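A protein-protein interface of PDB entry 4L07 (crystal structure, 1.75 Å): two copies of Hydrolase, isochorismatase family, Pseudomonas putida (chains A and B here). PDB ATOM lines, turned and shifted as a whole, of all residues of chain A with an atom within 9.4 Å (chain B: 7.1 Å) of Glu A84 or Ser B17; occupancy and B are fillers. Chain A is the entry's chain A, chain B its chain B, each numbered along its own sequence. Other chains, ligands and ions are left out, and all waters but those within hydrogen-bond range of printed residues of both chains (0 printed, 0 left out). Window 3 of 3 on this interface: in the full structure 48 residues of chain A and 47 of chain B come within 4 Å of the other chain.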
ATOM      1  N   TYR A  72      19.070 -10.538 -10.002  1.00  0.00           N
ATOM      2  CA  TYR A  72      19.746 -11.068 -11.197  1.00  0.00           C
ATOM      3  C   TYR A  72      21.256 -10.923 -11.175  1.00  0.00           C
ATOM      4  O   TYR A  72      21.794  -9.933 -10.682  1.00  0.00           O
ATOM      5  CB  TYR A  72      19.259 -10.367 -12.465  1.00  0.00           C
ATOM      6  CG  TYR A  72      17.774 -10.423 -12.636  1.00  0.00           C
ATOM      7  CD1 TYR A  72      17.147 -11.605 -13.021  1.00  0.00           C
ATOM      8  CD2 TYR A  72      16.991  -9.300 -12.389  1.00  0.00           C
ATOM      9  CE1 TYR A  72      15.771 -11.665 -13.163  1.00  0.00           C
ATOM     10  CE2 TYR A  72      15.616  -9.348 -12.530  1.00  0.00           C
ATOM     11  CZ  TYR A  72      15.016 -10.533 -12.922  1.00  0.00           C
ATOM     12  OH  TYR A  72      13.655 -10.597 -13.059  1.00  0.00           O
ATOM     13  N   GLU A  76      22.407 -12.981 -16.674  1.00  0.00           N
ATOM     14  CA  GLU A  76      21.033 -13.475 -16.806  1.00  0.00           C
ATOM     15  C   GLU A  76      20.127 -12.504 -17.560  1.00  0.00           C
ATOM     16  O   GLU A  76      19.150 -12.928 -18.190  1.00  0.00           O
ATOM     17  CB  GLU A  76      20.425 -13.770 -15.436  1.00  0.00           C
ATOM     18  CG  GLU A  76      20.993 -15.001 -14.749  1.00  0.00           C
ATOM     19  CD  GLU A  76      20.408 -15.231 -13.366  1.00  0.00           C
ATOM     20  OE1 GLU A  76      20.047 -16.386 -13.065  1.00  0.00           O
ATOM     21  OE2 GLU A  76      20.300 -14.267 -12.576  1.00  0.00           O
ATOM     22  N   ILE A  77      20.444 -11.210 -17.487  1.00  0.00           N
ATOM     23  CA  ILE A  77      19.584 -10.158 -18.062  1.00  0.00           C
ATOM     24  C   ILE A  77      19.196 -10.412 -19.538  1.00  0.00           C
ATOM     25  O   ILE A  77      18.004 -10.421 -19.867  1.00  0.00           O
ATOM     26  CB  ILE A  77      20.183  -8.732 -17.863  1.00  0.00           C
ATOM     27  CG1 ILE A  77      20.562  -8.470 -16.391  1.00  0.00           C
ATOM     28  CG2 ILE A  77      19.247  -7.656 -18.402  1.00  0.00           C
ATOM     29  CD1 ILE A  77      19.403  -8.307 -15.429  1.00  0.00           C
ATOM     30  N   PRO A  78      20.185 -10.662 -20.427  1.00  0.00           N
ATOM     31  CA  PRO A  78      19.809 -10.907 -21.825  1.00  0.00           C
ATOM     32  C   PRO A  78      19.129 -12.257 -22.085  1.00  0.00           C
ATOM     33  O   PRO A  78      18.571 -12.462 -23.164  1.00  0.00           O
ATOM     34  CB  PRO A  78      21.147 -10.818 -22.576  1.00  0.00           C
ATOM     35  CG  PRO A  78      22.183 -11.112 -21.548  1.00  0.00           C
ATOM     36  CD  PRO A  78      21.648 -10.566 -20.256  1.00  0.00           C
ATOM     37  N   MET A  79      19.161 -13.152 -21.100  1.00  0.00           N
ATOM     38  CA  MET A  79      18.613 -14.499 -21.259  1.00  0.00           C
ATOM     39  C   MET A  79      17.113 -14.598 -20.974  1.00  0.00           C
ATOM     40  O   MET A  79      16.468 -15.552 -21.405  1.00  0.00           O
ATOM     41  CB  MET A  79      19.345 -15.484 -20.345  1.00  0.00           C
ATOM     42  CG  MET A  79      20.853 -15.496 -20.510  1.00  0.00           C
ATOM     43  SD  MET A  79      21.544 -16.914 -19.637  1.00  0.00           S
ATOM     44  CE  MET A  79      23.278 -16.729 -20.027  1.00  0.00           C
ATOM     45  N   LEU A  80      16.570 -13.641 -20.228  1.00  0.00           N
ATOM     46  CA  LEU A  80      15.189 -13.751 -19.745  1.00  0.00           C
ATOM     47  C   LEU A  80      14.261 -12.734 -20.418  1.00  0.00           C
ATOM     48  O   LEU A  80      14.390 -11.526 -20.191  1.00  0.00           O
ATOM     49  CB  LEU A  80      15.134 -13.605 -18.223  1.00  0.00           C
ATOM     50  CG  LEU A  80      15.871 -14.635 -17.365  1.00  0.00           C
ATOM     51  CD1 LEU A  80      16.067 -14.115 -15.948  1.00  0.00           C
ATOM     52  CD2 LEU A  80      15.146 -15.980 -17.370  1.00  0.00           C
ATOM     53  N   PRO A  81      13.319 -13.219 -21.246  1.00  0.00           N
ATOM     54  CA  PRO A  81      12.481 -12.292 -22.004  1.00  0.00           C
ATOM     55  C   PRO A  81      11.549 -11.425 -21.155  1.00  0.00           C
ATOM     56  O   PRO A  81      11.088 -10.403 -21.645  1.00  0.00           O
ATOM     57  CB  PRO A  81      11.685 -13.205 -22.947  1.00  0.00           C
ATOM     58  CG  PRO A  81      11.699 -14.538 -22.286  1.00  0.00           C
ATOM     59  CD  PRO A  81      13.030 -14.627 -21.589  1.00  0.00           C
ATOM     60  N   TRP A  82      11.281 -11.805 -19.903  1.00  0.00           N
ATOM     61  CA  TRP A  82      10.490 -10.926 -19.037  1.00  0.00           C
ATOM     62  C   TRP A  82      11.122  -9.558 -18.910  1.00  0.00           C
ATOM     63  O   TRP A  82      10.420  -8.541 -18.847  1.00  0.00           O
ATOM     64  CB  TRP A  82      10.239 -11.554 -17.668  1.00  0.00           C
ATOM     65  CG  TRP A  82       9.335 -10.715 -16.804  1.00  0.00           C
ATOM     66  CD1 TRP A  82       8.074 -10.210 -17.129  1.00  0.00           C
ATOM     67  CD2 TRP A  82       9.588 -10.265 -15.435  1.00  0.00           C
ATOM     68  NE1 TRP A  82       7.553  -9.483 -16.086  1.00  0.00           N
ATOM     69  CE2 TRP A  82       8.412  -9.482 -15.036  1.00  0.00           C
ATOM     70  CE3 TRP A  82      10.636 -10.423 -14.531  1.00  0.00           C
ATOM     71  CZ2 TRP A  82       8.313  -8.886 -13.785  1.00  0.00           C
ATOM     72  CZ3 TRP A  82      10.520  -9.824 -13.269  1.00  0.00           C
ATOM     73  CH2 TRP A  82       9.386  -9.074 -12.908  1.00  0.00           C
ATOM     74  N   LEU A  83      12.453  -9.523 -18.905  1.00  0.00           N
ATOM     75  CA  LEU A  83      13.204  -8.264 -18.774  1.00  0.00           C
ATOM     76  C   LEU A  83      13.192  -7.395 -20.038  1.00  0.00           C
ATOM     77  O   LEU A  83      13.556  -6.214 -19.984  1.00  0.00           O
ATOM     78  CB  LEU A  83      14.642  -8.531 -18.305  1.00  0.00           C
ATOM     79  CG  LEU A  83      14.879  -9.131 -16.913  1.00  0.00           C
ATOM     80  CD1 LEU A  83      14.047  -8.443 -15.843  1.00  0.00           C
ATOM     81  CD2 LEU A  83      14.582 -10.617 -16.903  1.00  0.00           C
ATOM     82  N   GLU A  84      12.778  -7.976 -21.166  1.00  0.00           N
ATOM     83  CA  GLU A  84      12.512  -7.195 -22.377  1.00  0.00           C
ATOM     84  C   GLU A  84      11.251  -6.339 -22.194  1.00  0.00           C
ATOM     85  O   GLU A  84      11.259  -5.143 -22.505  1.00  0.00           O
ATOM     86  CB  GLU A  84      12.383  -8.108 -23.600  1.00  0.00           C
ATOM     87  CG  GLU A  84      11.960  -7.398 -24.880  1.00  0.00           C
ATOM     88  CD  GLU A  84      11.820  -8.347 -26.054  1.00  0.00           C
ATOM     89  OE1 GLU A  84      11.171  -9.402 -25.902  1.00  0.00           O
ATOM     90  OE2 GLU A  84      12.363  -8.039 -27.133  1.00  0.00           O
ATOM     91  N   LYS A  85      10.181  -6.949 -21.679  1.00  0.00           N
ATOM     92  CA  LYS A  85       8.938  -6.229 -21.370  1.00  0.00           C
ATOM     93  C   LYS A  85       9.090  -5.310 -20.160  1.00  0.00           C
ATOM     94  O   LYS A  85       8.776  -4.115 -20.226  1.00  0.00           O
ATOM     95  CB  LYS A  85       7.773  -7.201 -21.100  1.00  0.00           C
ATOM     96  CG  LYS A  85       7.166  -7.880 -22.321  1.00  0.00           C
ATOM     97  CD  LYS A  85       6.527  -6.915 -23.321  1.00  0.00           C
ATOM     98  CE  LYS A  85       5.508  -5.972 -22.693  1.00  0.00           C
ATOM     99  NZ  LYS A  85       4.834  -5.134 -23.726  1.00  0.00           N
ATOM    100  N   SER A  86       9.509  -5.898 -19.053  1.00  0.00           N
ATOM    101  CA  SER A  86       9.659  -5.183 -17.811  1.00  0.00           C
ATOM    102  C   SER A  86      11.134  -4.837 -17.557  1.00  0.00           C
ATOM    103  O   SER A  86      11.783  -5.427 -16.727  1.00  0.00           O
ATOM    104  CB  SER A  86       9.026  -5.997 -16.680  1.00  0.00           C
ATOM    105  OG  SER A  86       7.670  -6.313 -16.946  1.00  0.00           O
ATOM    106  N   SER A  87      11.638  -3.860 -18.285  1.00  0.00           N
ATOM    107  CA  SER A  87      13.081  -3.583 -18.323  1.00  0.00           C
ATOM    108  C   SER A  87      13.608  -2.909 -17.058  1.00  0.00           C
ATOM    109  O   SER A  87      14.808  -2.968 -16.780  1.00  0.00           O
ATOM    110  CB  SER A  87      13.447  -2.766 -19.566  1.00  0.00           C
ATOM    111  OG  SER A  87      12.886  -1.466 -19.501  1.00  0.00           O
ATOM    112  N   GLY A  88      12.712  -2.277 -16.297  1.00  0.00           N
ATOM    113  CA  GLY A  88      13.063  -1.704 -14.992  1.00  0.00           C
ATOM    114  C   GLY A  88      13.593  -2.742 -14.021  1.00  0.00           C
ATOM    115  O   GLY A  88      14.391  -2.438 -13.131  1.00  0.00           O
ATOM    116  N   MET A  89      13.157  -3.984 -14.207  1.00  0.00           N
ATOM    117  CA  MET A  89      13.573  -5.080 -13.345  1.00  0.00           C
ATOM    118  C   MET A  89      15.063  -5.413 -13.461  1.00  0.00           C
ATOM    119  O   MET A  89      15.634  -6.023 -12.557  1.00  0.00           O
ATOM    120  CB  MET A  89      12.722  -6.326 -13.620  1.00  0.00           C
ATOM    121  CG  MET A  89      11.230  -6.083 -13.452  1.00  0.00           C
ATOM    122  SD  MET A  89      10.759  -5.687 -11.761  1.00  0.00           S
ATOM    123  CE  MET A  89       9.012  -5.359 -11.992  1.00  0.00           C
ATOM    124  N   ALA A  90      15.687  -5.010 -14.562  1.00  0.00           N
ATOM    125  CA  ALA A  90      17.113  -5.283 -14.772  1.00  0.00           C
ATOM    126  C   ALA A  90      18.011  -4.572 -13.750  1.00  0.00           C
ATOM    127  O   ALA A  90      19.176  -4.937 -13.585  1.00  0.00           O
ATOM    128  CB  ALA A  90      17.519  -4.927 -16.197  1.00  0.00           C
ATOM    129  N   GLY B  11       9.866   1.266 -16.195  1.00  0.00           N
ATOM    130  CA  GLY B  11      10.453   0.453 -17.268  1.00  0.00           C
ATOM    131  C   GLY B  11       9.526  -0.563 -17.916  1.00  0.00           C
ATOM    132  O   GLY B  11       9.998  -1.491 -18.588  1.00  0.00           O
ATOM    133  N   PHE B  12       8.218  -0.388 -17.718  1.00  0.00           N
ATOM    134  CA  PHE B  12       7.193  -1.270 -18.309  1.00  0.00           C
ATOM    135  C   PHE B  12       6.764  -0.844 -19.716  1.00  0.00           C
ATOM    136  O   PHE B  12       7.012   0.288 -20.142  1.00  0.00           O
ATOM    137  CB  PHE B  12       5.943  -1.311 -17.423  1.00  0.00           C
ATOM    138  CG  PHE B  12       6.156  -1.948 -16.081  1.00  0.00           C
ATOM    139  CD1 PHE B  12       6.456  -3.308 -15.970  1.00  0.00           C
ATOM    140  CD2 PHE B  12       5.998  -1.205 -14.922  1.00  0.00           C
ATOM    141  CE1 PHE B  12       6.634  -3.896 -14.723  1.00  0.00           C
ATOM    142  CE2 PHE B  12       6.179  -1.782 -13.669  1.00  0.00           C
ATOM    143  CZ  PHE B  12       6.492  -3.130 -13.565  1.00  0.00           C
ATOM    144  N   GLY B  13       6.109  -1.760 -20.429  1.00  0.00           N
ATOM    145  CA  GLY B  13       5.445  -1.444 -21.697  1.00  0.00           C
ATOM    146  C   GLY B  13       6.329  -1.455 -22.929  1.00  0.00           C
ATOM    147  O   GLY B  13       5.906  -1.013 -24.000  1.00  0.00           O
ATOM    148  N   ASN B  14       7.552  -1.967 -22.792  1.00  0.00           N
ATOM    149  CA  ASN B  14       8.467  -2.071 -23.927  1.00  0.00           C
ATOM    150  C   ASN B  14       7.952  -3.076 -24.954  1.00  0.00           C
ATOM    151  O   ASN B  14       7.304  -4.058 -24.578  1.00  0.00           O
ATOM    152  CB  ASN B  14       9.861  -2.491 -23.456  1.00  0.00           C
ATOM    153  CG  ASN B  14      10.469  -1.502 -22.484  1.00  0.00           C
ATOM    154  OD1 ASN B  14      10.844  -0.395 -22.863  1.00  0.00           O
ATOM    155  ND2 ASN B  14      10.570  -1.898 -21.227  1.00  0.00           N
ATOM    156  N   PRO B  15       8.237  -2.838 -26.245  1.00  0.00           N
ATOM    157  CA  PRO B  15       7.802  -3.780 -27.275  1.00  0.00           C
ATOM    158  C   PRO B  15       8.590  -5.095 -27.242  1.00  0.00           C
ATOM    159  O   PRO B  15       9.741  -5.132 -26.794  1.00  0.00           O
ATOM    160  CB  PRO B  15       8.091  -3.026 -28.578  1.00  0.00           C
ATOM    161  CG  PRO B  15       9.227  -2.120 -28.237  1.00  0.00           C
ATOM    162  CD  PRO B  15       8.939  -1.675 -26.828  1.00  0.00           C
ATOM    163  N   VAL B  16       7.967  -6.168 -27.704  1.00  0.00           N
ATOM    164  CA  VAL B  16       8.683  -7.431 -27.860  1.00  0.00           C
ATOM    165  C   VAL B  16       9.352  -7.480 -29.230  1.00  0.00           C
ATOM    166  O   VAL B  16       8.714  -7.240 -30.257  1.00  0.00           O
ATOM    167  CB  VAL B  16       7.770  -8.660 -27.622  1.00  0.00           C
ATOM    168  CG1 VAL B  16       6.457  -8.506 -28.338  1.00  0.00           C
ATOM    169  CG2 VAL B  16       8.434  -9.947 -28.087  1.00  0.00           C
ATOM    170  N   SER B  17      10.652  -7.763 -29.232  1.00  0.00           N
ATOM    171  CA  SER B  17      11.369  -8.046 -30.461  1.00  0.00           C
ATOM    172  C   SER B  17      11.066  -9.496 -30.805  1.00  0.00           C
ATOM    173  O   SER B  17      11.566 -10.410 -30.156  1.00  0.00           O
ATOM    174  CB  SER B  17      12.873  -7.833 -30.275  1.00  0.00           C
ATOM    175  OG  SER B  17      13.556  -8.021 -31.498  1.00  0.00           O
ATOM    176  N   ARG B  18      10.219  -9.696 -31.809  1.00  0.00           N
ATOM    177  CA  ARG B  18       9.693 -11.030 -32.111  1.00  0.00           C
ATOM    178  C   ARG B  18      10.761 -11.962 -32.672  1.00  0.00           C
ATOM    179  O   ARG B  18      11.667 -11.521 -33.384  1.00  0.00           O
ATOM    180  CB  ARG B  18       8.525 -10.920 -33.088  1.00  0.00           C
ATOM    181  CG  ARG B  18       7.329 -10.201 -32.487  1.00  0.00           C
ATOM    182  CD  ARG B  18       6.250  -9.935 -33.517  1.00  0.00           C
ATOM    183  NE  ARG B  18       5.272  -8.992 -32.989  1.00  0.00           N
ATOM    184  CZ  ARG B  18       4.107  -8.700 -33.565  1.00  0.00           C
ATOM    185  NH1 ARG B  18       3.737  -9.292 -34.693  1.00  0.00           N
ATOM    186  NH2 ARG B  18       3.302  -7.817 -32.998  1.00  0.00           N
ATOM    187  N   GLY B  19      10.648 -13.246 -32.333  1.00  0.00           N
ATOM    188  CA  GLY B  19      11.574 -14.267 -32.819  1.00  0.00           C
ATOM    189  C   GLY B  19      11.138 -14.867 -34.142  1.00  0.00           C
ATOM    190  O   GLY B  19      10.268 -14.329 -34.829  1.00  0.00           O
ATOM    191  N   VAL B  20      11.745 -15.994 -34.499  1.00  0.00           N
ATOM    192  CA  VAL B  20      11.526 -16.599 -35.814  1.00  0.00           C
ATOM    193  C   VAL B  20      11.032 -18.051 -35.747  1.00  0.00           C
ATOM    194  O   VAL B  20      10.968 -18.741 -36.773  1.00  0.00           O
ATOM    195  CB  VAL B  20      12.787 -16.490 -36.716  1.00  0.00           C
ATOM    196  CG1 VAL B  20      13.165 -15.031 -36.944  1.00  0.00           C
ATOM    197  CG2 VAL B  20      13.955 -17.265 -36.119  1.00  0.00           C
ATOM    198  N   ASP B 137      10.581 -19.848 -29.910  1.00  0.00           N
ATOM    199  CA  ASP B 137      11.048 -18.636 -29.235  1.00  0.00           C
ATOM    200  C   ASP B 137       9.951 -17.610 -28.950  1.00  0.00           C
ATOM    201  O   ASP B 137      10.124 -16.729 -28.103  1.00  0.00           O
ATOM    202  CB  ASP B 137      12.248 -17.995 -29.965  1.00  0.00           C
ATOM    203  CG  ASP B 137      11.952 -17.622 -31.419  1.00  0.00           C
ATOM    204  OD1 ASP B 137      10.775 -17.525 -31.827  1.00  0.00           O
ATOM    205  OD2 ASP B 137      12.932 -17.405 -32.171  1.00  0.00           O
ATOM    206  N   THR B 138       8.821 -17.743 -29.644  1.00  0.00           N
ATOM    207  CA  THR B 138       7.728 -16.776 -29.540  1.00  0.00           C
ATOM    208  C   THR B 138       6.391 -17.516 -29.561  1.00  0.00           C
ATOM    209  O   THR B 138       6.142 -18.331 -30.452  1.00  0.00           O
ATOM    210  CB  THR B 138       7.773 -15.778 -30.713  1.00  0.00           C
ATOM    211  OG1 THR B 138       9.102 -15.258 -30.843  1.00  0.00           O
ATOM    212  CG2 THR B 138       6.786 -14.621 -30.507  1.00  0.00           C
ATOM    213  N   LYS B 163       8.984 -15.357 -25.601  1.00  0.00           N
ATOM    214  CA  LYS B 163       8.372 -14.065 -25.883  1.00  0.00           C
ATOM    215  C   LYS B 163       6.889 -14.296 -26.188  1.00  0.00           C
ATOM    216  O   LYS B 163       6.527 -15.330 -26.747  1.00  0.00           O
ATOM    217  CB  LYS B 163       9.059 -13.406 -27.073  1.00  0.00           C
ATOM    218  CG  LYS B 163      10.494 -12.994 -26.789  1.00  0.00           C
ATOM    219  CD  LYS B 163      11.305 -12.989 -28.072  1.00  0.00           C
ATOM    220  CE  LYS B 163      12.730 -12.513 -27.829  1.00  0.00           C
ATOM    221  NZ  LYS B 163      12.840 -11.030 -27.803  1.00  0.00           N
ATOM    222  N   VAL B 164       6.045 -13.342 -25.800  1.00  0.00           N
ATOM    223  CA  VAL B 164       4.587 -13.537 -25.845  1.00  0.00           C
ATOM    224  C   VAL B 164       3.835 -12.466 -26.623  1.00  0.00           C
ATOM    225  O   VAL B 164       4.010 -11.267 -26.385  1.00  0.00           O
ATOM    226  CB  VAL B 164       3.974 -13.614 -24.426  1.00  0.00           C
ATOM    227  CG1 VAL B 164       2.468 -13.856 -24.493  1.00  0.00           C
ATOM    228  CG2 VAL B 164       4.635 -14.715 -23.614  1.00  0.00           C
ATOM    229  N   LEU B 165       2.974 -12.929 -27.528  1.00  0.00           N
ATOM    230  CA  LEU B 165       2.056 -12.081 -28.269  1.00  0.00           C
ATOM    231  C   LEU B 165       0.631 -12.527 -27.958  1.00  0.00           C
ATOM    232  O   LEU B 165       0.343 -13.718 -27.889  1.00  0.00           O
ATOM    233  CB  LEU B 165       2.317 -12.161 -29.775  1.00  0.00           C
ATOM    234  CG  LEU B 165       3.740 -11.873 -30.263  1.00  0.00           C
ATOM    235  CD1 LEU B 165       3.836 -12.162 -31.752  1.00  0.00           C
ATOM    236  CD2 LEU B 165       4.160 -10.436 -29.978  1.00  0.00           C
ATOM    237  N   LYS B 189       3.565  -5.670 -18.641  1.00  0.00           N
ATOM    238  CA  LYS B 189       4.548  -6.480 -17.918  1.00  0.00           C
ATOM    239  C   LYS B 189       4.993  -7.783 -18.576  1.00  0.00           C
ATOM    240  O   LYS B 189       6.075  -8.273 -18.262  1.00  0.00           O
ATOM    241  CB  LYS B 189       4.044  -6.788 -16.498  1.00  0.00           C
ATOM    242  CG  LYS B 189       3.636  -5.566 -15.685  1.00  0.00           C
ATOM    243  CD  LYS B 189       3.447  -5.899 -14.212  1.00  0.00           C
ATOM    244  CE  LYS B 189       2.952  -4.685 -13.420  1.00  0.00           C
ATOM    245  NZ  LYS B 189       2.564  -5.076 -12.028  1.00  0.00           N
ATOM    246  N   ASP B 192       3.131  -8.549 -25.706  1.00  0.00           N
ATOM    247  CA  ASP B 192       2.530  -7.516 -26.549  1.00  0.00           C
ATOM    248  C   ASP B 192       1.099  -7.872 -26.899  1.00  0.00           C
ATOM    249  O   ASP B 192       0.841  -8.932 -27.461  1.00  0.00           O
ATOM    250  CB  ASP B 192       3.337  -7.286 -27.823  1.00  0.00           C
ATOM    251  CG  ASP B 192       4.459  -6.267 -27.632  1.00  0.00           C
ATOM    252  OD1 ASP B 192       4.592  -5.700 -26.523  1.00  0.00           O
ATOM    253  OD2 ASP B 192       5.212  -6.027 -28.606  1.00  0.00           O
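Of chain B, only Asn B14, Pro B15, Val B16, Ser B17 and Lys B163 come within 4 Å of Glu A84. Of the printed residues of chain B, Ser A86 touches Gly B11 (3.7 Å), Phe B12 (3.4 Å) and Lys B189 (2.8 Å). Printed residues of chain A within 4 Å of Asn B14: Glu A84, Lys A85 and Ser A87. Of chain A, only Glu A84 comes within 4 Å of Val B16. Ser B17 touches one residue of chain A. Asp B137 touches none of the printed residues of chain A. Printed residues of chain A within 4 Å of Lys B163: Glu A84 (3.0 Å). Of the printed residues of chain A, Lys B189 touches Trp A82 (2.9 Å), Lys A85 (3.5 Å) and Ser A86 (2.8 Å). The nearest residue of chain B that does not touch Glu A84 is Arg B18 (5.4 Å). The nearest residue of chain A that does not touch Ser B17 is Lys A85 (7.3 Å).
Asn B14 touches Glu A84 (CB to O, 3.1 Å). Pro B15 touches Glu A84 (O to CG, 3.7 Å). Val B16 touches Glu A84. Lys A85 touches Phe B12 (O to CA, 3.8 Å). Gly B13 touches Lys A85. O of Lys B189 touches CB of Lys A85, 3.5 Å away. Ser A86 touches Gly B11 (C to O, 3.7 Å). CD1 of Phe B12 touches OG of Ser A86, 3.4 Å away. Gly B11 touches Gly A88. Phe B12 touches Met A89 (CZ to CE, 3.7 Å).
O of Asp B137 is in hydrogen-bond range of N of Lys B163 (3.1 Å). The backbone carbonyl oxygen of Gly B11 is in hydrogen-bond range of the side-chain amide nitrogen of Asn B14, at 2.7 Å. O of Ser B17 lies within hydrogen-bond range of NZ of Lys B163, 2.7 Å away. OG of Ser A86 lies within hydrogen-bond range of NE1 of Trp A82 (3.3 Å). O of Val B164 lies within hydrogen-bond range of N of Asp B192 (2.9 Å). The backbone NH (N) of Val B16 sits close to the side-chain carboxylate (OD2) of Asp B192 (2.9 Å).
No position is printed for both chains. Of the 19 pairs that touch across the chains among the printed residues, none has its exchanged pair printed and touching as well.
The indole nitrogen (NE1) of Trp A82 lies within hydrogen-bond range of the backbone carbonyl oxygen (O) of Lys B189, 2.9 Å away. OG of Ser A86 sits at hydrogen-bond distance from O of Lys B189. The backbone carbonyl oxygen of Lys A85 lies close to the backbone carbonyl oxygen of Gly B11 (3.3 Å). N of Ser A87 lies within hydrogen-bond range of O of Gly B11, at 2.9 Å. The side-chain hydroxyl (OG) of Ser A87 lies within hydrogen-bond range of the side-chain amide nitrogen (ND2) of Asn B14, 2.9 Å away. O of Asn B14 is in hydrogen-bond range of NZ of Lys A85, 2.8 Å away. The side-chain amino group of Lys B163 is in salt-bridge range of the side-chain carboxylate of Glu A84 (3.0 Å). N of Ser B17 sits at hydrogen-bond distance from OE2 of Glu A84 (2.7 Å). NZ of Lys A85 lies within salt-bridge range of OD1 of Asp B192 (2.9 Å).
Of the 17 printed residues of chain B, 10 touch a printed residue of chain A. Among the printed residues, Asp or Glu carboxylates within 4 Å of a Lys or Arg side-chain nitrogen of the other chain: Glu A84 with Lys B163 (3.0 Å) and Lys A85 with Asp B192 (2.9 Å).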
